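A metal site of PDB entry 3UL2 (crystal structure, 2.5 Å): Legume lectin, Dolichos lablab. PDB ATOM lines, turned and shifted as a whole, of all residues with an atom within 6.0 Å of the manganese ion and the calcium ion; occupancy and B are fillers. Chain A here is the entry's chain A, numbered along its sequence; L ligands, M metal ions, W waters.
The calcium ion is bound by water W2 (2.2 Å), OD2 of Asp 156 (2.2 Å), OD1 of Asn 152 (2.3 Å), O of Phe 150 (2.4 Å), water W3 (2.4 Å), OD1 of Asp 148 (2.5 Å) and OD2 of Asp 148 (2.6 Å).
The calcium ion has seven donor atoms within binding distance.
Within 4 Å of the calcium ion: Asp 148, Phe 150, Asn 152 and Asp 156.
OD1 of Asp 156 binds the manganese ion, 2.1 Å away.
Water W4 is bound to the manganese ion, 2.1 Å away.
The manganese ion is bound by NE2 of His 161 (2.2 Å).
Water W1 binds the manganese ion, at 2.2 Å.
The manganese ion is bound by OE2 of Glu 146, at 2.2 Å.
The manganese ion is bound by the side-chain carboxylate (OD2) of Asp 148.
The manganese ion has six donor atoms within binding distance.
The side-chain carboxylate (OD1) of Asp 156 lies close to the indole nitrogen (NE1) of Trp 155 (3.5 Å).
OE2 of Glu 146 sits close to OG of Ser 171 (3.3 Å).
The side-chain carboxylate of Glu 146 lies close to the side-chain carboxylate of Asp 165.
Within 4 Å of the manganese ion: Glu 146, Asp 148, Asp 156 and His 161.
The nearest printed residue that does not touch the manganese ion is Ser 171 (4.2 Å).
Water W1 lies within hydrogen-bond range of OE1 of Glu 146 (2.8 Å), O of Ile 169 (2.8 Å) and NE1 of Trp 155 (3.2 Å).
Water W3 lies within hydrogen-bond range of O of Gly 126 and NE1 of Trp 155.
The side-chain amide nitrogen (ND2) of Asn 152 sits at hydrogen-bond distance from an oxygen (O3) of the ligand.
An oxygen (O3) of the ligand lies within hydrogen-bond range of the backbone NH (N) of Gly 126 (3.0 Å).
The side-chain carboxylate (OD1) of Asp 108 is in hydrogen-bond range of an oxygen (O3) of the ligand (2.6 Å).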
ATOM      1  N   ASP A 108      -4.212 -14.724 -14.382  1.00  0.00           N
ATOM      2  CA  ASP A 108      -4.276 -13.557 -15.250  1.00  0.00           C
ATOM      3  C   ASP A 108      -5.444 -13.606 -16.222  1.00  0.00           C
ATOM      4  O   ASP A 108      -5.972 -12.565 -16.613  1.00  0.00           O
ATOM      5  CB  ASP A 108      -2.961 -13.404 -16.023  1.00  0.00           C
ATOM      6  CG  ASP A 108      -1.982 -12.506 -15.317  1.00  0.00           C
ATOM      7  OD1 ASP A 108      -2.123 -11.278 -15.428  1.00  0.00           O
ATOM      8  OD2 ASP A 108      -1.073 -13.028 -14.661  1.00  0.00           O
ATOM      9  N   GLY A 126       0.541 -11.722 -17.455  1.00  0.00           N
ATOM     10  CA  GLY A 126      -0.381 -10.863 -18.204  1.00  0.00           C
ATOM     11  C   GLY A 126      -0.355 -11.028 -19.720  1.00  0.00           C
ATOM     12  O   GLY A 126      -1.285 -10.594 -20.399  1.00  0.00           O
ATOM     13  N   LEU A 128      -0.468 -13.921 -21.091  1.00  0.00           N
ATOM     14  CA  LEU A 128      -1.361 -15.062 -21.293  1.00  0.00           C
ATOM     15  C   LEU A 128      -0.763 -16.238 -22.078  1.00  0.00           C
ATOM     16  O   LEU A 128      -1.494 -17.099 -22.562  1.00  0.00           O
ATOM     17  CB  LEU A 128      -2.692 -14.593 -21.925  1.00  0.00           C
ATOM     18  CG  LEU A 128      -3.468 -13.489 -21.193  1.00  0.00           C
ATOM     19  CD1 LEU A 128      -4.570 -12.927 -22.078  1.00  0.00           C
ATOM     20  CD2 LEU A 128      -4.034 -13.989 -19.866  1.00  0.00           C
ATOM     21  N   GLU A 146      -9.402 -12.787 -25.711  1.00  0.00           N
ATOM     22  CA  GLU A 146      -8.976 -12.932 -24.326  1.00  0.00           C
ATOM     23  C   GLU A 146     -10.119 -12.659 -23.358  1.00  0.00           C
ATOM     24  O   GLU A 146     -11.033 -11.872 -23.641  1.00  0.00           O
ATOM     25  CB  GLU A 146      -7.782 -12.030 -24.008  1.00  0.00           C
ATOM     26  CG  GLU A 146      -8.058 -10.535 -24.161  1.00  0.00           C
ATOM     27  CD  GLU A 146      -6.949  -9.667 -23.597  1.00  0.00           C
ATOM     28  OE1 GLU A 146      -5.765  -9.975 -23.816  1.00  0.00           O
ATOM     29  OE2 GLU A 146      -7.281  -8.672 -22.926  1.00  0.00           O
ATOM     30  N   ASP A 148      -9.852 -11.477 -19.704  1.00  0.00           N
ATOM     31  CA  ASP A 148      -8.748 -10.929 -18.919  1.00  0.00           C
ATOM     32  C   ASP A 148      -9.195 -10.546 -17.500  1.00  0.00           C
ATOM     33  O   ASP A 148      -9.893  -9.552 -17.310  1.00  0.00           O
ATOM     34  CB  ASP A 148      -8.169  -9.731 -19.667  1.00  0.00           C
ATOM     35  CG  ASP A 148      -6.799  -9.314 -19.141  1.00  0.00           C
ATOM     36  OD1 ASP A 148      -6.450  -9.652 -17.988  1.00  0.00           O
ATOM     37  OD2 ASP A 148      -6.067  -8.635 -19.905  1.00  0.00           O
ATOM     38  N   THR A 149      -8.737 -11.347 -16.539  1.00  0.00           N
ATOM     39  CA  THR A 149      -9.133 -11.221 -15.127  1.00  0.00           C
ATOM     40  C   THR A 149      -8.311 -10.174 -14.377  1.00  0.00           C
ATOM     41  O   THR A 149      -8.637  -9.830 -13.242  1.00  0.00           O
ATOM     42  CB  THR A 149      -8.917 -12.563 -14.363  1.00  0.00           C
ATOM     43  OG1 THR A 149      -9.723 -13.603 -14.948  1.00  0.00           O
ATOM     44  CG2 THR A 149      -9.249 -12.430 -12.888  1.00  0.00           C
ATOM     45  N   PHE A 150      -7.249  -9.671 -15.000  1.00  0.00           N
ATOM     46  CA  PHE A 150      -6.291  -8.823 -14.277  1.00  0.00           C
ATOM     47  C   PHE A 150      -5.880  -7.534 -14.977  1.00  0.00           C
ATOM     48  O   PHE A 150      -5.473  -7.538 -16.137  1.00  0.00           O
ATOM     49  CB  PHE A 150      -5.038  -9.634 -13.892  1.00  0.00           C
ATOM     50  CG  PHE A 150      -4.075  -8.868 -13.026  1.00  0.00           C
ATOM     51  CD1 PHE A 150      -3.053  -8.117 -13.598  1.00  0.00           C
ATOM     52  CD2 PHE A 150      -4.200  -8.882 -11.650  1.00  0.00           C
ATOM     53  CE1 PHE A 150      -2.167  -7.403 -12.820  1.00  0.00           C
ATOM     54  CE2 PHE A 150      -3.319  -8.184 -10.858  1.00  0.00           C
ATOM     55  CZ  PHE A 150      -2.296  -7.439 -11.444  1.00  0.00           C
ATOM     56  N   TYR A 151      -5.923  -6.441 -14.214  1.00  0.00           N
ATOM     57  CA  TYR A 151      -5.609  -5.089 -14.681  1.00  0.00           C
ATOM     58  C   TYR A 151      -4.102  -4.906 -14.820  1.00  0.00           C
ATOM     59  O   TYR A 151      -3.411  -4.638 -13.845  1.00  0.00           O
ATOM     60  CB  TYR A 151      -6.217  -4.093 -13.689  1.00  0.00           C
ATOM     61  CG  TYR A 151      -6.092  -2.605 -13.990  1.00  0.00           C
ATOM     62  CD1 TYR A 151      -6.088  -2.127 -15.288  1.00  0.00           C
ATOM     63  CD2 TYR A 151      -6.043  -1.680 -12.946  1.00  0.00           C
ATOM     64  CE1 TYR A 151      -5.998  -0.756 -15.550  1.00  0.00           C
ATOM     65  CE2 TYR A 151      -5.959  -0.321 -13.181  1.00  0.00           C
ATOM     66  CZ  TYR A 151      -5.937   0.136 -14.485  1.00  0.00           C
ATOM     67  OH  TYR A 151      -5.851   1.498 -14.729  1.00  0.00           O
ATOM     68  N   ASN A 152      -3.608  -5.065 -16.043  1.00  0.00           N
ATOM     69  CA  ASN A 152      -2.180  -4.873 -16.321  1.00  0.00           C
ATOM     70  C   ASN A 152      -1.811  -3.426 -16.651  1.00  0.00           C
ATOM     71  O   ASN A 152      -0.628  -3.085 -16.713  1.00  0.00           O
ATOM     72  CB  ASN A 152      -1.704  -5.795 -17.444  1.00  0.00           C
ATOM     73  CG  ASN A 152      -1.414  -7.204 -16.965  1.00  0.00           C
ATOM     74  OD1 ASN A 152      -2.207  -8.117 -17.172  1.00  0.00           O
ATOM     75  ND2 ASN A 152      -0.273  -7.383 -16.320  1.00  0.00           N
ATOM     76  N   TRP A 155      -1.327  -1.696 -20.434  1.00  0.00           N
ATOM     77  CA  TRP A 155      -2.088  -1.830 -21.668  1.00  0.00           C
ATOM     78  C   TRP A 155      -3.603  -2.057 -21.461  1.00  0.00           C
ATOM     79  O   TRP A 155      -4.387  -1.847 -22.392  1.00  0.00           O
ATOM     80  CB  TRP A 155      -1.498  -2.950 -22.541  1.00  0.00           C
ATOM     81  CG  TRP A 155      -1.431  -4.295 -21.881  1.00  0.00           C
ATOM     82  CD1 TRP A 155      -2.430  -5.224 -21.838  1.00  0.00           C
ATOM     83  CD2 TRP A 155      -0.311  -4.874 -21.192  1.00  0.00           C
ATOM     84  NE1 TRP A 155      -2.002  -6.351 -21.161  1.00  0.00           N
ATOM     85  CE2 TRP A 155      -0.711  -6.157 -20.758  1.00  0.00           C
ATOM     86  CE3 TRP A 155       0.988  -4.433 -20.908  1.00  0.00           C
ATOM     87  CZ2 TRP A 155       0.147  -7.011 -20.055  1.00  0.00           C
ATOM     88  CZ3 TRP A 155       1.845  -5.282 -20.192  1.00  0.00           C
ATOM     89  CH2 TRP A 155       1.419  -6.552 -19.780  1.00  0.00           C
ATOM     90  N   ASP A 156      -4.002  -2.467 -20.256  1.00  0.00           N
ATOM     91  CA  ASP A 156      -5.383  -2.897 -20.001  1.00  0.00           C
ATOM     92  C   ASP A 156      -6.361  -1.775 -19.657  1.00  0.00           C
ATOM     93  O   ASP A 156      -5.969  -0.740 -19.125  1.00  0.00           O
ATOM     94  CB  ASP A 156      -5.411  -3.944 -18.884  1.00  0.00           C
ATOM     95  CG  ASP A 156      -5.118  -5.340 -19.391  1.00  0.00           C
ATOM     96  OD1 ASP A 156      -5.345  -5.616 -20.590  1.00  0.00           O
ATOM     97  OD2 ASP A 156      -4.675  -6.179 -18.576  1.00  0.00           O
ATOM     98  N   PRO A 157      -7.660  -1.990 -19.970  1.00  0.00           N
ATOM     99  CA  PRO A 157      -8.726  -1.142 -19.414  1.00  0.00           C
ATOM    100  C   PRO A 157      -8.858  -1.386 -17.911  1.00  0.00           C
ATOM    101  O   PRO A 157      -8.285  -2.338 -17.389  1.00  0.00           O
ATOM    102  CB  PRO A 157      -9.993  -1.627 -20.140  1.00  0.00           C
ATOM    103  CG  PRO A 157      -9.506  -2.410 -21.319  1.00  0.00           C
ATOM    104  CD  PRO A 157      -8.204  -3.001 -20.887  1.00  0.00           C
ATOM    105  N   HIS A 161     -12.286  -7.616 -18.607  1.00  0.00           N
ATOM    106  CA  HIS A 161     -12.697  -7.360 -19.971  1.00  0.00           C
ATOM    107  C   HIS A 161     -12.546  -8.567 -20.886  1.00  0.00           C
ATOM    108  O   HIS A 161     -11.749  -9.476 -20.630  1.00  0.00           O
ATOM    109  CB  HIS A 161     -11.922  -6.175 -20.544  1.00  0.00           C
ATOM    110  CG  HIS A 161     -10.440  -6.318 -20.469  1.00  0.00           C
ATOM    111  ND1 HIS A 161      -9.723  -6.095 -19.317  1.00  0.00           N
ATOM    112  CD2 HIS A 161      -9.529  -6.671 -21.416  1.00  0.00           C
ATOM    113  CE1 HIS A 161      -8.430  -6.307 -19.544  1.00  0.00           C
ATOM    114  NE2 HIS A 161      -8.287  -6.649 -20.812  1.00  0.00           N
ATOM    115  N   ASP A 165      -7.276  -9.703 -29.538  1.00  0.00           N
ATOM    116  CA  ASP A 165      -5.838  -9.526 -29.628  1.00  0.00           C
ATOM    117  C   ASP A 165      -5.286  -9.908 -30.999  1.00  0.00           C
ATOM    118  O   ASP A 165      -5.406 -11.060 -31.432  1.00  0.00           O
ATOM    119  CB  ASP A 165      -5.140 -10.370 -28.552  1.00  0.00           C
ATOM    120  CG  ASP A 165      -5.522  -9.971 -27.133  1.00  0.00           C
ATOM    121  OD1 ASP A 165      -6.216  -8.945 -26.938  1.00  0.00           O
ATOM    122  OD2 ASP A 165      -5.131 -10.697 -26.197  1.00  0.00           O
ATOM    123  N   ILE A 169      -0.626  -8.134 -27.027  1.00  0.00           N
ATOM    124  CA  ILE A 169      -1.416  -8.276 -25.799  1.00  0.00           C
ATOM    125  C   ILE A 169      -2.304  -7.042 -25.585  1.00  0.00           C
ATOM    126  O   ILE A 169      -3.261  -7.072 -24.806  1.00  0.00           O
ATOM    127  CB  ILE A 169      -0.544  -8.576 -24.540  1.00  0.00           C
ATOM    128  CG1 ILE A 169      -1.393  -9.075 -23.369  1.00  0.00           C
ATOM    129  CG2 ILE A 169       0.275  -7.358 -24.116  1.00  0.00           C
ATOM    130  CD1 ILE A 169      -2.078 -10.405 -23.588  1.00  0.00           C
ATOM    131  N   SER A 171      -5.088  -5.259 -26.707  1.00  0.00           N
ATOM    132  CA  SER A 171      -6.271  -5.513 -27.530  1.00  0.00           C
ATOM    133  C   SER A 171      -6.593  -4.350 -28.459  1.00  0.00           C
ATOM    134  O   SER A 171      -6.442  -3.185 -28.081  1.00  0.00           O
ATOM    135  CB  SER A 171      -7.473  -5.802 -26.636  1.00  0.00           C
ATOM    136  OG  SER A 171      -7.213  -6.851 -25.725  1.00  0.00           O
ATOM    137  N   THR A 174     -11.915  -3.752 -26.777  1.00  0.00           N
ATOM    138  CA  THR A 174     -12.354  -4.486 -25.587  1.00  0.00           C
ATOM    139  C   THR A 174     -13.813  -4.178 -25.252  1.00  0.00           C
ATOM    140  O   THR A 174     -14.422  -3.265 -25.846  1.00  0.00           O
ATOM    141  CB  THR A 174     -11.495  -4.164 -24.321  1.00  0.00           C
ATOM    142  OG1 THR A 174     -11.657  -2.790 -23.952  1.00  0.00           O
ATOM    143  CG2 THR A 174     -10.014  -4.466 -24.536  1.00  0.00           C
HETATM  144  C1  LIG L   1       2.540  -9.000 -12.326  1.00  0.00           C
HETATM  145  C2  LIG L   1       2.079  -9.402 -13.728  1.00  0.00           C
HETATM  146  C3  LIG L   1       0.546  -9.487 -13.786  1.00  0.00           C
HETATM  147  C4  LIG L   1      -0.007 -10.334 -12.641  1.00  0.00           C
HETATM  148  C5  LIG L   1       0.561  -9.800 -11.322  1.00  0.00           C
HETATM  149  C6  LIG L   1       0.032 -10.551 -10.104  1.00  0.00           C
HETATM  150  O1  LIG L   1       3.943  -9.125 -12.249  1.00  0.00           O
HETATM  151  O2  LIG L   1       2.553  -8.482 -14.687  1.00  0.00           O
HETATM  152  O3  LIG L   1       0.142 -10.024 -15.035  1.00  0.00           O
HETATM  153  O4  LIG L   1       0.343 -11.679 -12.807  1.00  0.00           O
HETATM  154  O5  LIG L   1       1.972  -9.859 -11.360  1.00  0.00           O
HETATM  155  O6  LIG L   1       0.474  -9.880  -8.953  1.00  0.00           O
HETATM  156 MN    MN M   1      -6.325  -7.141 -21.613  1.00  0.00          MN
HETATM  157 CA    CA M   2      -4.287  -8.316 -18.043  1.00  0.00          CA
HETATM  158  O   HOH W   1      -4.425  -7.968 -22.427  1.00  0.00           O
HETATM  159  O   HOH W   2      -3.859 -10.331 -17.308  1.00  0.00           O
HETATM  160  O   HOH W   3      -3.337  -8.766 -20.256  1.00  0.00           O
HETATM  161  O   HOH W   4      -7.028  -5.868 -23.132  1.00  0.00           O
